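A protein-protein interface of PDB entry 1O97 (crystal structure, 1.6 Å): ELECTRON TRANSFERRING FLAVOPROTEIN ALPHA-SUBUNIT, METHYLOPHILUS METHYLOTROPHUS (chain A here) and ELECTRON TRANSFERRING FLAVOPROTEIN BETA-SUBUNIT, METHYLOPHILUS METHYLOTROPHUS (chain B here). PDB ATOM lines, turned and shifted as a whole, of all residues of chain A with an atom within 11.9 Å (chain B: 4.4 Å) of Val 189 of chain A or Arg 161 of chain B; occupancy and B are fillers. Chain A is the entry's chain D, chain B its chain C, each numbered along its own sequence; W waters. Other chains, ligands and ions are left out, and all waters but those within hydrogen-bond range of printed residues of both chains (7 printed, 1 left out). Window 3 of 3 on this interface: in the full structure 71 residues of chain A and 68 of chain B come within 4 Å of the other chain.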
ATOM      1  N   ARG A  10     -31.207  16.125  -5.320  1.00  0.00           N
ATOM      2  CA  ARG A  10     -31.220  15.652  -6.709  1.00  0.00           C
ATOM      3  C   ARG A  10     -32.525  14.867  -6.900  1.00  0.00           C
ATOM      4  O   ARG A  10     -32.881  14.095  -6.026  1.00  0.00           O
ATOM      5  CB  ARG A  10     -30.028  14.697  -6.898  1.00  0.00           C
ATOM      6  CG  ARG A  10     -29.974  13.981  -8.214  1.00  0.00           C
ATOM      7  CD  ARG A  10     -28.670  13.222  -8.415  1.00  0.00           C
ATOM      8  NE  ARG A  10     -27.544  14.142  -8.436  1.00  0.00           N
ATOM      9  CZ  ARG A  10     -26.396  13.933  -7.795  1.00  0.00           C
ATOM     10  NH1 ARG A  10     -26.200  12.823  -7.065  1.00  0.00           N
ATOM     11  NH2 ARG A  10     -25.451  14.879  -7.876  1.00  0.00           N
ATOM     12  N   ARG A  11     -33.209  15.069  -8.022  1.00  0.00           N
ATOM     13  CA  ARG A  11     -34.382  14.223  -8.351  1.00  0.00           C
ATOM     14  C   ARG A  11     -35.412  14.250  -7.213  1.00  0.00           C
ATOM     15  O   ARG A  11     -35.947  13.203  -6.799  1.00  0.00           O
ATOM     16  CB  ARG A  11     -33.987  12.753  -8.652  1.00  0.00           C
ATOM     17  CG  ARG A  11     -33.350  12.452  -9.986  1.00  0.00           C
ATOM     18  CD  ARG A  11     -33.588  10.944 -10.416  1.00  0.00           C
ATOM     19  NE  ARG A  11     -33.422  10.011  -9.294  1.00  0.00           N
ATOM     20  CZ  ARG A  11     -33.384   8.684  -9.409  1.00  0.00           C
ATOM     21  NH1 ARG A  11     -33.453   8.101 -10.609  1.00  0.00           N
ATOM     22  NH2 ARG A  11     -33.235   7.940  -8.320  1.00  0.00           N
ATOM     23  N   ASP A  69     -32.209  21.266 -10.906  1.00  0.00           N
ATOM     24  CA  ASP A  69     -31.102  20.597 -10.223  1.00  0.00           C
ATOM     25  C   ASP A  69     -29.766  21.254 -10.497  1.00  0.00           C
ATOM     26  O   ASP A  69     -29.654  22.261 -11.202  1.00  0.00           O
ATOM     27  CB  ASP A  69     -31.104  19.108 -10.614  1.00  0.00           C
ATOM     28  CG  ASP A  69     -32.178  18.316  -9.870  1.00  0.00           C
ATOM     29  OD1 ASP A  69     -32.815  18.865  -8.921  1.00  0.00           O
ATOM     30  OD2 ASP A  69     -32.457  17.127 -10.142  1.00  0.00           O
ATOM     31  N   PHE A  70     -28.713  20.691  -9.918  1.00  0.00           N
ATOM     32  CA  PHE A  70     -27.416  21.362  -9.995  1.00  0.00           C
ATOM     33  C   PHE A  70     -26.980  21.928 -11.344  1.00  0.00           C
ATOM     34  O   PHE A  70     -26.978  21.228 -12.376  1.00  0.00           O
ATOM     35  CB  PHE A  70     -26.344  20.404  -9.502  1.00  0.00           C
ATOM     36  CG  PHE A  70     -24.942  20.960  -9.621  1.00  0.00           C
ATOM     37  CD1 PHE A  70     -24.476  21.925  -8.723  1.00  0.00           C
ATOM     38  CD2 PHE A  70     -24.098  20.547 -10.652  1.00  0.00           C
ATOM     39  CE1 PHE A  70     -23.174  22.445  -8.875  1.00  0.00           C
ATOM     40  CE2 PHE A  70     -22.857  21.047 -10.813  1.00  0.00           C
ATOM     41  CZ  PHE A  70     -22.356  22.026  -9.935  1.00  0.00           C
ATOM     42  N   PRO A  72     -23.451  24.319 -12.458  1.00  0.00           N
ATOM     43  CA  PRO A  72     -22.248  24.951 -11.879  1.00  0.00           C
ATOM     44  C   PRO A  72     -22.242  26.462 -11.901  1.00  0.00           C
ATOM     45  O   PRO A  72     -21.718  27.086 -10.970  1.00  0.00           O
ATOM     46  CB  PRO A  72     -21.076  24.423 -12.729  1.00  0.00           C
ATOM     47  CG  PRO A  72     -21.665  23.796 -13.932  1.00  0.00           C
ATOM     48  CD  PRO A  72     -23.112  23.457 -13.625  1.00  0.00           C
ATOM     49  N   VAL A  97     -19.883  14.906  -6.437  1.00  0.00           N
ATOM     50  CA  VAL A  97     -19.764  15.217  -7.846  1.00  0.00           C
ATOM     51  C   VAL A  97     -20.256  16.624  -8.201  1.00  0.00           C
ATOM     52  O   VAL A  97     -19.615  17.318  -8.989  1.00  0.00           O
ATOM     53  CB  VAL A  97     -20.450  14.110  -8.672  1.00  0.00           C
ATOM     54  CG1 VAL A  97     -20.457  14.479 -10.081  1.00  0.00           C
ATOM     55  CG2 VAL A  97     -19.667  12.755  -8.439  1.00  0.00           C
ATOM     56  N   ASP A  98     -21.348  17.056  -7.578  1.00  0.00           N
ATOM     57  CA  ASP A  98     -21.840  18.419  -7.852  1.00  0.00           C
ATOM     58  C   ASP A  98     -20.797  19.476  -7.415  1.00  0.00           C
ATOM     59  O   ASP A  98     -20.420  20.395  -8.168  1.00  0.00           O
ATOM     60  CB  ASP A  98     -23.165  18.728  -7.121  1.00  0.00           C
ATOM     61  CG  ASP A  98     -24.418  18.028  -7.769  1.00  0.00           C
ATOM     62  OD1 ASP A  98     -24.334  17.391  -8.868  1.00  0.00           O
ATOM     63  OD2 ASP A  98     -25.541  18.112  -7.210  1.00  0.00           O
ATOM     64  N   GLY A 101     -18.013  20.335  -9.620  1.00  0.00           N
ATOM     65  CA  GLY A 101     -18.265  21.203 -10.766  1.00  0.00           C
ATOM     66  C   GLY A 101     -18.099  22.689 -10.481  1.00  0.00           C
ATOM     67  O   GLY A 101     -18.051  23.471 -11.442  1.00  0.00           O
ATOM     68  N   SER A 183     -24.474  26.171 -19.648  1.00  0.00           N
ATOM     69  CA  SER A 183     -24.898  24.804 -19.900  1.00  0.00           C
ATOM     70  C   SER A 183     -26.378  24.650 -19.566  1.00  0.00           C
ATOM     71  O   SER A 183     -26.993  25.511 -18.870  1.00  0.00           O
ATOM     72  CB  SER A 183     -23.959  23.776 -19.170  1.00  0.00           C
ATOM     73  OG  SER A 183     -24.020  23.826 -17.745  1.00  0.00           O
ATOM     74  N   GLN A 184     -26.975  23.595 -20.109  1.00  0.00           N
ATOM     75  CA  GLN A 184     -28.356  23.249 -19.784  1.00  0.00           C
ATOM     76  C   GLN A 184     -28.489  21.784 -19.494  1.00  0.00           C
ATOM     77  O   GLN A 184     -28.047  20.943 -20.288  1.00  0.00           O
ATOM     78  CB  GLN A 184     -29.256  23.573 -21.007  1.00  0.00           C
ATOM     79  CG  GLN A 184     -30.690  23.124 -20.871  1.00  0.00           C
ATOM     80  CD  GLN A 184     -31.463  23.979 -19.888  1.00  0.00           C
ATOM     81  OE1 GLN A 184     -31.296  25.213 -19.859  1.00  0.00           O
ATOM     82  NE2 GLN A 184     -32.319  23.333 -19.082  1.00  0.00           N
ATOM     83  N   ASN A 185     -29.136  21.462 -18.382  1.00  0.00           N
ATOM     84  CA  ASN A 185     -29.340  20.071 -17.953  1.00  0.00           C
ATOM     85  C   ASN A 185     -30.387  19.391 -18.819  1.00  0.00           C
ATOM     86  O   ASN A 185     -31.430  20.020 -19.120  1.00  0.00           O
ATOM     87  CB  ASN A 185     -29.744  19.969 -16.515  1.00  0.00           C
ATOM     88  CG  ASN A 185     -28.621  20.386 -15.543  1.00  0.00           C
ATOM     89  OD1 ASN A 185     -27.417  20.329 -15.884  1.00  0.00           O
ATOM     90  ND2 ASN A 185     -29.015  20.768 -14.330  1.00  0.00           N
ATOM     91  N   LYS A 186     -30.090  18.168 -19.235  1.00  0.00           N
ATOM     92  CA  LYS A 186     -31.036  17.372 -20.048  1.00  0.00           C
ATOM     93  C   LYS A 186     -31.447  16.125 -19.288  1.00  0.00           C
ATOM     94  O   LYS A 186     -31.646  16.165 -18.093  1.00  0.00           O
ATOM     95  CB  LYS A 186     -30.461  17.087 -21.438  1.00  0.00           C
ATOM     96  CG  LYS A 186     -29.893  18.254 -22.168  1.00  0.00           C
ATOM     97  CD  LYS A 186     -30.880  19.420 -22.234  1.00  0.00           C
ATOM     98  CE  LYS A 186     -31.452  19.642 -23.556  1.00  0.00           C
ATOM     99  NZ  LYS A 186     -31.915  21.071 -23.674  1.00  0.00           N
ATOM    100  N   ASP A 187     -31.592  14.971 -19.928  1.00  0.00           N
ATOM    101  CA  ASP A 187     -32.137  13.844 -19.206  1.00  0.00           C
ATOM    102  C   ASP A 187     -31.223  13.249 -18.106  1.00  0.00           C
ATOM    103  O   ASP A 187     -30.003  13.294 -18.306  1.00  0.00           O
ATOM    104  CB  ASP A 187     -32.361  12.676 -20.230  1.00  0.00           C
ATOM    105  CG  ASP A 187     -33.600  12.869 -21.089  1.00  0.00           C
ATOM    106  OD1 ASP A 187     -34.512  13.616 -20.659  1.00  0.00           O
ATOM    107  OD2 ASP A 187     -33.674  12.361 -22.245  1.00  0.00           O
ATOM    108  N   TYR A 188     -31.764  12.687 -17.039  1.00  0.00           N
ATOM    109  CA  TYR A 188     -31.007  11.699 -16.274  1.00  0.00           C
ATOM    110  C   TYR A 188     -31.010  10.402 -17.026  1.00  0.00           C
ATOM    111  O   TYR A 188     -31.936  10.160 -17.819  1.00  0.00           O
ATOM    112  CB  TYR A 188     -31.583  11.508 -14.863  1.00  0.00           C
ATOM    113  CG  TYR A 188     -31.327  12.713 -13.928  1.00  0.00           C
ATOM    114  CD1 TYR A 188     -32.381  13.523 -13.468  1.00  0.00           C
ATOM    115  CD2 TYR A 188     -30.025  13.051 -13.573  1.00  0.00           C
ATOM    116  CE1 TYR A 188     -32.158  14.632 -12.572  1.00  0.00           C
ATOM    117  CE2 TYR A 188     -29.777  14.180 -12.717  1.00  0.00           C
ATOM    118  CZ  TYR A 188     -30.825  14.940 -12.233  1.00  0.00           C
ATOM    119  OH  TYR A 188     -30.554  16.016 -11.450  1.00  0.00           O
ATOM    120  N   VAL A 189     -29.971   9.568 -16.829  1.00  0.00           N
ATOM    121  CA  VAL A 189     -29.880   8.327 -17.600  1.00  0.00           C
ATOM    122  C   VAL A 189     -29.355   7.223 -16.731  1.00  0.00           C
ATOM    123  O   VAL A 189     -28.378   7.440 -15.996  1.00  0.00           O
ATOM    124  CB  VAL A 189     -28.931   8.487 -18.819  1.00  0.00           C
ATOM    125  CG1 VAL A 189     -28.847   7.193 -19.604  1.00  0.00           C
ATOM    126  CG2 VAL A 189     -29.386   9.584 -19.720  1.00  0.00           C
ATOM    127  N   GLU A 190     -30.003   6.052 -16.814  1.00  0.00           N
ATOM    128  CA  GLU A 190     -29.561   4.813 -16.179  1.00  0.00           C
ATOM    129  C   GLU A 190     -29.098   3.917 -17.308  1.00  0.00           C
ATOM    130  O   GLU A 190     -29.902   3.551 -18.171  1.00  0.00           O
ATOM    131  CB  GLU A 190     -30.744   4.123 -15.531  1.00  0.00           C
ATOM    132  CG  GLU A 190     -30.367   3.044 -14.547  1.00  0.00           C
ATOM    133  CD  GLU A 190     -30.424   3.544 -13.116  1.00  0.00           C
ATOM    134  OE1 GLU A 190     -30.698   4.765 -12.909  1.00  0.00           O
ATOM    135  OE2 GLU A 190     -30.205   2.712 -12.201  1.00  0.00           O
ATOM    136  N   VAL A 191     -27.817   3.576 -17.314  1.00  0.00           N
ATOM    137  CA  VAL A 191     -27.189   2.895 -18.447  1.00  0.00           C
ATOM    138  C   VAL A 191     -27.611   1.419 -18.552  1.00  0.00           C
ATOM    139  O   VAL A 191     -28.055   0.814 -17.567  1.00  0.00           O
ATOM    140  CB  VAL A 191     -25.654   3.142 -18.438  1.00  0.00           C
ATOM    141  CG1 VAL A 191     -24.851   1.930 -18.888  1.00  0.00           C
ATOM    142  CG2 VAL A 191     -25.351   4.372 -19.296  1.00  0.00           C
ATOM    143  N   GLY A 192     -27.513   0.882 -19.769  1.00  0.00           N
ATOM    144  CA  GLY A 192     -28.024  -0.450 -20.084  1.00  0.00           C
ATOM    145  C   GLY A 192     -26.985  -1.527 -19.843  1.00  0.00           C
ATOM    146  O   GLY A 192     -26.197  -1.364 -18.925  1.00  0.00           O
ATOM    147  N   ARG A 236     -14.488  -0.818  -9.479  1.00  0.00           N
ATOM    148  CA  ARG A 236     -14.711  -0.108 -10.718  1.00  0.00           C
ATOM    149  C   ARG A 236     -13.913  -0.556 -11.965  1.00  0.00           C
ATOM    150  O   ARG A 236     -14.513  -0.618 -13.050  1.00  0.00           O
ATOM    151  CB  ARG A 236     -14.521   1.398 -10.505  1.00  0.00           C
ATOM    152  CG  ARG A 236     -14.956   2.216 -11.663  1.00  0.00           C
ATOM    153  CD  ARG A 236     -14.460   3.612 -11.554  1.00  0.00           C
ATOM    154  NE  ARG A 236     -14.892   4.279 -12.768  1.00  0.00           N
ATOM    155  CZ  ARG A 236     -15.941   5.090 -12.815  1.00  0.00           C
ATOM    156  NH1 ARG A 236     -16.562   5.476 -11.686  1.00  0.00           N
ATOM    157  NH2 ARG A 236     -16.273   5.634 -13.976  1.00  0.00           N
ATOM    158  N   ASP A 240     -15.636  -0.950 -15.642  1.00  0.00           N
ATOM    159  CA  ASP A 240     -15.173  -0.032 -16.693  1.00  0.00           C
ATOM    160  C   ASP A 240     -14.681  -0.846 -17.889  1.00  0.00           C
ATOM    161  O   ASP A 240     -14.913  -0.484 -19.009  1.00  0.00           O
ATOM    162  CB  ASP A 240     -14.044   0.915 -16.239  1.00  0.00           C
ATOM    163  CG  ASP A 240     -14.547   2.158 -15.466  1.00  0.00           C
ATOM    164  OD1 ASP A 240     -15.779   2.388 -15.377  1.00  0.00           O
ATOM    165  OD2 ASP A 240     -13.725   2.943 -14.925  1.00  0.00           O
ATOM    166  N   LYS A 246     -22.101  -3.179 -14.809  1.00  0.00           N
ATOM    167  CA  LYS A 246     -22.049  -2.002 -13.919  1.00  0.00           C
ATOM    168  C   LYS A 246     -22.920  -2.242 -12.695  1.00  0.00           C
ATOM    169  O   LYS A 246     -22.615  -1.779 -11.587  1.00  0.00           O
ATOM    170  CB  LYS A 246     -22.418  -0.709 -14.665  1.00  0.00           C
ATOM    171  CG  LYS A 246     -21.350  -0.166 -15.635  1.00  0.00           C
ATOM    172  CD  LYS A 246     -20.296   0.759 -14.957  1.00  0.00           C
ATOM    173  N   SER A 247     -23.951  -3.069 -12.867  1.00  0.00           N
ATOM    174  CA  SER A 247     -24.796  -3.506 -11.745  1.00  0.00           C
ATOM    175  C   SER A 247     -24.087  -4.258 -10.600  1.00  0.00           C
ATOM    176  O   SER A 247     -24.625  -4.349  -9.489  1.00  0.00           O
ATOM    177  CB  SER A 247     -26.053  -4.309 -12.234  1.00  0.00           C
ATOM    178  OG  SER A 247     -25.711  -5.578 -12.783  1.00  0.00           O
ATOM    179  N   SER A 253     -19.838   5.394  -7.089  1.00  0.00           N
ATOM    180  CA  SER A 253     -20.644   5.551  -8.318  1.00  0.00           C
ATOM    181  C   SER A 253     -21.293   4.222  -8.783  1.00  0.00           C
ATOM    182  O   SER A 253     -21.826   4.127  -9.899  1.00  0.00           O
ATOM    183  CB  SER A 253     -19.824   6.245  -9.393  1.00  0.00           C
ATOM    184  OG  SER A 253     -18.696   5.480  -9.679  1.00  0.00           O
ATOM    185  N   GLY A 254     -21.236   3.215  -7.917  1.00  0.00           N
ATOM    186  CA  GLY A 254     -21.855   1.919  -8.071  1.00  0.00           C
ATOM    187  C   GLY A 254     -22.876   1.811  -6.963  1.00  0.00           C
ATOM    188  O   GLY A 254     -23.589   2.799  -6.689  1.00  0.00           O
ATOM    189  N   LYS A 255     -22.920   0.656  -6.322  1.00  0.00           N
ATOM    190  CA  LYS A 255     -23.866   0.384  -5.255  1.00  0.00           C
ATOM    191  C   LYS A 255     -23.223   0.370  -3.883  1.00  0.00           C
ATOM    192  O   LYS A 255     -22.048  -0.009  -3.708  1.00  0.00           O
ATOM    193  CB  LYS A 255     -24.597  -0.955  -5.484  1.00  0.00           C
ATOM    194  CG  LYS A 255     -25.142  -1.150  -6.890  1.00  0.00           C
ATOM    195  CD  LYS A 255     -25.815   0.093  -7.493  1.00  0.00           C
ATOM    196  CE  LYS A 255     -25.273   0.367  -8.930  1.00  0.00           C
ATOM    197  NZ  LYS A 255     -26.242   1.116  -9.782  1.00  0.00           N
ATOM    198  N   VAL B 145     -16.462  15.560 -14.153  1.00  0.00           N
ATOM    199  CA  VAL B 145     -16.767  14.127 -14.045  1.00  0.00           C
ATOM    200  C   VAL B 145     -17.529  13.609 -15.280  1.00  0.00           C
ATOM    201  O   VAL B 145     -18.630  12.999 -15.149  1.00  0.00           O
ATOM    202  CB  VAL B 145     -17.435  13.657 -12.727  1.00  0.00           C
ATOM    203  CG1 VAL B 145     -17.295  12.137 -12.471  1.00  0.00           C
ATOM    204  CG2 VAL B 145     -16.885  14.367 -11.438  1.00  0.00           C
ATOM    205  N   VAL B 146     -16.924  13.906 -16.417  1.00  0.00           N
ATOM    206  CA  VAL B 146     -17.476  13.598 -17.754  1.00  0.00           C
ATOM    207  C   VAL B 146     -17.200  12.145 -18.130  1.00  0.00           C
ATOM    208  O   VAL B 146     -16.040  11.717 -18.243  1.00  0.00           O
ATOM    209  CB  VAL B 146     -16.975  14.606 -18.762  1.00  0.00           C
ATOM    210  CG1 VAL B 146     -17.433  14.206 -20.212  1.00  0.00           C
ATOM    211  CG2 VAL B 146     -17.483  16.025 -18.398  1.00  0.00           C
ATOM    212  N   ALA B 147     -18.303  11.398 -18.307  1.00  0.00           N
ATOM    213  CA  ALA B 147     -18.275   9.969 -18.695  1.00  0.00           C
ATOM    214  C   ALA B 147     -18.603   9.714 -20.159  1.00  0.00           C
ATOM    215  O   ALA B 147     -18.442   8.588 -20.650  1.00  0.00           O
ATOM    216  CB  ALA B 147     -19.177   9.174 -17.812  1.00  0.00           C
ATOM    217  N   ASP B 148     -19.060  10.745 -20.849  1.00  0.00           N
ATOM    218  CA  ASP B 148     -19.376  10.647 -22.294  1.00  0.00           C
ATOM    219  C   ASP B 148     -19.332  12.010 -22.924  1.00  0.00           C
ATOM    220  O   ASP B 148     -19.725  12.977 -22.304  1.00  0.00           O
ATOM    221  CB  ASP B 148     -20.779  10.062 -22.525  1.00  0.00           C
ATOM    222  CG  ASP B 148     -21.002   9.683 -23.970  1.00  0.00           C
ATOM    223  OD1 ASP B 148     -21.843  10.355 -24.653  1.00  0.00           O
ATOM    224  OD2 ASP B 148     -20.321   8.781 -24.539  1.00  0.00           O
ATOM    225  N   ILE B 160     -22.553  16.301 -23.057  1.00  0.00           N
ATOM    226  CA  ILE B 160     -21.785  15.426 -22.178  1.00  0.00           C
ATOM    227  C   ILE B 160     -22.696  14.674 -21.273  1.00  0.00           C
ATOM    228  O   ILE B 160     -23.896  15.030 -21.114  1.00  0.00           O
ATOM    229  CB  ILE B 160     -20.722  16.292 -21.379  1.00  0.00           C
ATOM    230  CG1 ILE B 160     -21.449  17.310 -20.478  1.00  0.00           C
ATOM    231  CG2 ILE B 160     -19.802  16.975 -22.391  1.00  0.00           C
ATOM    232  CD1 ILE B 160     -21.383  16.892 -19.075  1.00  0.00           C
ATOM    233  N   ARG B 161     -22.210  13.571 -20.717  1.00  0.00           N
ATOM    234  CA  ARG B 161     -22.876  12.887 -19.617  1.00  0.00           C
ATOM    235  C   ARG B 161     -21.986  12.923 -18.410  1.00  0.00           C
ATOM    236  O   ARG B 161     -20.815  12.468 -18.473  1.00  0.00           O
ATOM    237  CB  ARG B 161     -23.237  11.440 -19.943  1.00  0.00           C
ATOM    238  CG  ARG B 161     -24.367  11.369 -21.004  1.00  0.00           C
ATOM    239  CD  ARG B 161     -24.636   9.969 -21.530  1.00  0.00           C
ATOM    240  NE  ARG B 161     -25.844   9.993 -22.347  1.00  0.00           N
ATOM    241  CZ  ARG B 161     -26.597   8.918 -22.623  1.00  0.00           C
ATOM    242  NH1 ARG B 161     -26.328   7.728 -22.105  1.00  0.00           N
ATOM    243  NH2 ARG B 161     -27.677   9.080 -23.372  1.00  0.00           N
ATOM    244  N   ARG B 162     -22.517  13.471 -17.326  1.00  0.00           N
ATOM    245  CA  ARG B 162     -21.692  13.466 -16.103  1.00  0.00           C
ATOM    246  C   ARG B 162     -22.096  12.333 -15.181  1.00  0.00           C
ATOM    247  O   ARG B 162     -23.276  11.977 -15.091  1.00  0.00           O
ATOM    248  CB  ARG B 162     -21.552  14.898 -15.591  1.00  0.00           C
ATOM    249  CG  ARG B 162     -22.670  15.424 -14.869  1.00  0.00           C
ATOM    250  CD  ARG B 162     -22.449  16.851 -14.203  1.00  0.00           C
ATOM    251  NE  ARG B 162     -23.702  17.065 -13.503  1.00  0.00           N
ATOM    252  CZ  ARG B 162     -23.922  17.079 -12.182  1.00  0.00           C
ATOM    253  NH1 ARG B 162     -22.934  16.979 -11.267  1.00  0.00           N
ATOM    254  NH2 ARG B 162     -25.164  17.235 -11.750  1.00  0.00           N
ATOM    255  N   GLU B 163     -21.106  11.700 -14.535  1.00  0.00           N
ATOM    256  CA  GLU B 163     -21.350  10.524 -13.742  1.00  0.00           C
ATOM    257  C   GLU B 163     -21.645  10.828 -12.287  1.00  0.00           C
ATOM    258  O   GLU B 163     -20.774  11.420 -11.586  1.00  0.00           O
ATOM    259  CB  GLU B 163     -20.152   9.562 -13.862  1.00  0.00           C
ATOM    260  CG  GLU B 163     -20.362   8.271 -13.119  1.00  0.00           C
ATOM    261  CD  GLU B 163     -19.043   7.520 -12.967  1.00  0.00           C
ATOM    262  OE1 GLU B 163     -18.283   7.787 -12.005  1.00  0.00           O
ATOM    263  OE2 GLU B 163     -18.731   6.710 -13.857  1.00  0.00           O
ATOM    264  N   MET B 168     -26.159   6.645 -11.754  1.00  0.00           N
ATOM    265  CA  MET B 168     -26.893   7.474 -12.701  1.00  0.00           C
ATOM    266  C   MET B 168     -25.981   8.463 -13.416  1.00  0.00           C
ATOM    267  O   MET B 168     -24.954   8.907 -12.857  1.00  0.00           O
ATOM    268  CB  MET B 168     -28.111   8.128 -12.059  1.00  0.00           C
ATOM    269  CG  MET B 168     -27.850   9.292 -11.145  1.00  0.00           C
ATOM    270  SD  MET B 168     -29.373   9.682 -10.289  1.00  0.00           S
ATOM    271  CE  MET B 168     -30.539   9.746 -11.581  1.00  0.00           C
ATOM    272  N   LEU B 169     -26.325   8.824 -14.644  1.00  0.00           N
ATOM    273  CA  LEU B 169     -25.657   9.891 -15.349  1.00  0.00           C
ATOM    274  C   LEU B 169     -26.622  11.048 -15.552  1.00  0.00           C
ATOM    275  O   LEU B 169     -27.847  10.874 -15.480  1.00  0.00           O
ATOM    276  CB  LEU B 169     -25.169   9.404 -16.722  1.00  0.00           C
ATOM    277  CG  LEU B 169     -24.466   8.042 -16.709  1.00  0.00           C
ATOM    278  CD1 LEU B 169     -24.179   7.591 -18.150  1.00  0.00           C
ATOM    279  CD2 LEU B 169     -23.163   8.128 -15.891  1.00  0.00           C
ATOM    280  N   GLN B 170     -26.062  12.188 -15.848  1.00  0.00           N
ATOM    281  CA  GLN B 170     -26.849  13.357 -16.273  1.00  0.00           C
ATOM    282  C   GLN B 170     -26.338  13.872 -17.595  1.00  0.00           C
ATOM    283  O   GLN B 170     -25.156  14.218 -17.756  1.00  0.00           O
ATOM    284  CB  GLN B 170     -26.979  14.411 -15.158  1.00  0.00           C
ATOM    285  CG  GLN B 170     -27.837  15.593 -15.617  1.00  0.00           C
ATOM    286  CD  GLN B 170     -27.833  16.726 -14.610  1.00  0.00           C
ATOM    287  OE1 GLN B 170     -28.907  17.241 -14.214  1.00  0.00           O
ATOM    288  NE2 GLN B 170     -26.640  17.147 -14.215  1.00  0.00           N
ATOM    289  N   GLU B 171     -27.170  13.918 -18.643  1.00  0.00           N
ATOM    290  CA  GLU B 171     -26.838  14.589 -19.852  1.00  0.00           C
ATOM    291  C   GLU B 171     -26.942  16.097 -19.663  1.00  0.00           C
ATOM    292  O   GLU B 171     -27.880  16.590 -19.019  1.00  0.00           O
ATOM    293  CB  GLU B 171     -27.761  14.135 -21.001  1.00  0.00           C
ATOM    294  CG  GLU B 171     -27.566  12.710 -21.453  1.00  0.00           C
ATOM    295  CD  GLU B 171     -28.054  12.520 -22.883  1.00  0.00           C
ATOM    296  OE1 GLU B 171     -28.979  11.709 -23.106  1.00  0.00           O
ATOM    297  OE2 GLU B 171     -27.556  13.224 -23.782  1.00  0.00           O
HETATM  298  O   HOH W   1     -20.052  17.602 -11.771  1.00  0.00           O
HETATM  299  O   HOH W   2     -28.018  16.456 -10.186  1.00  0.00           O
HETATM  300  O   HOH W   3     -31.705  10.577 -23.083  1.00  0.00           O
HETATM  301  O   HOH W   4     -30.026   7.292  -8.915  1.00  0.00           O
HETATM  302  O   HOH W   5     -19.297   4.033 -12.473  1.00  0.00           O
HETATM  303  O   HOH W   6     -25.203  20.118 -14.296  1.00  0.00           O
HETATM  304  O   HOH W   7     -31.443  16.365 -15.305  1.00  0.00           O
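Water W7 lies within hydrogen-bond range of the backbone carbonyl oxygen of Lys 186 of chain A (2.8 Å) and the side-chain amide oxygen of Gln 170 of chain B (2.9 Å). Water W2 lies within hydrogen-bond range of OH of Tyr 188 of chain A (2.9 Å), NE of Arg 10 of chain A (2.9 Å) and NH2 of Arg 162 of chain B (3.3 Å).
Of the 12 printed residues of chain B, 8 touch a printed residue of chain A. Hydrophobic or aromatic side chains of chain B that line the printed part of chain A: Val 145, Met 168 and Leu 169. Along chain B the printed residues that touch a printed residue of chain A span positions 145 to 171. Of the 25 printed residues of chain A, 12 touch a printed residue of chain B. Hydrophobic or aromatic side chains of chain A within 4 Å of the printed part of chain B: Phe 70, Val 97, Tyr 188, Val 189 and Val 191. Among the printed residues, 20 pairs touch across the chains.
Arg 161 of chain B touches just one residue of chain A: Val 189. No residue of chain A comes within 4 Å of Ala 147 of chain B. No residue of chain A comes within 4 Å of Asp 148 of chain B. No residue of chain A comes within 4 Å of Ile 160 of chain B. Of the printed residues of chain B, Tyr 188 of chain A touches Met 168 (3.9 Å), Leu 169 (3.4 Å) and Gln 170 (3.4 Å). Printed residues of chain B within 4 Å of Lys 186 of chain A: Glu 171. Of the printed residues of chain A, Gln 170 of chain B touches Asn 185, Asp 187 and Tyr 188. Arg 10 of chain A touches none of the printed residues of chain B.
O of Val 145 of chain B sits at hydrogen-bond distance from N of Glu 163 of chain B, 2.9 Å away. The backbone NH of Arg 162 of chain B lies within hydrogen-bond range of the backbone carbonyl oxygen of Gln 170 of chain B (2.8 Å).
O of Asp 187 of chain A sits at hydrogen-bond distance from N of Glu 171 of chain B (2.9 Å). NH2 of Arg 236 of chain A is in salt-bridge range of OE2 of Glu 163 of chain B (2.7 Å). The backbone NH of Lys 186 of chain A lies within hydrogen-bond range of the backbone carbonyl oxygen of Glu 171 of chain B, at 2.7 Å. The backbone NH of Leu 169 of chain B sits at hydrogen-bond distance from the backbone carbonyl oxygen of Val 189 of chain A, at 2.8 Å. The guanidinium group (NH1) of Arg 162 of chain B is in salt-bridge range of the side-chain carboxylate (OD1) of Asp 98 of chain A (2.8 Å). The side-chain amide oxygen (OE1) of Gln 170 of chain B is in hydrogen-bond range of the side-chain hydroxyl (OH) of Tyr 188 of chain A, 3.4 Å away. OE1 of Glu 163 of chain B sits at hydrogen-bond distance from OG of Ser 253 of chain A (3.3 Å).
Among the printed residues, merely in contact across the chains: Arg 11 of chain A with Met 168 of chain B, Phe 70 of chain A with Arg 162 of chain B, Val 97 of chain A with Val 145 of chain B, Val 97 of chain A with Arg 162 of chain B, Val 97 of chain A with Glu 163 of chain B, Asn 185 of chain A with Gln 170 of chain B, Asn 185 of chain A with Glu 171 of chain B, Asp 187 of chain A with Gln 170 of chain B, Tyr 188 of chain A with Met 168 of chain B, Tyr 188 of chain A with Leu 169 of chain B, Val 189 of chain A with Arg 161 of chain B, Val 189 of chain A with Met 168 of chain B and Val 191 of chain A with Leu 169 of chain B.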
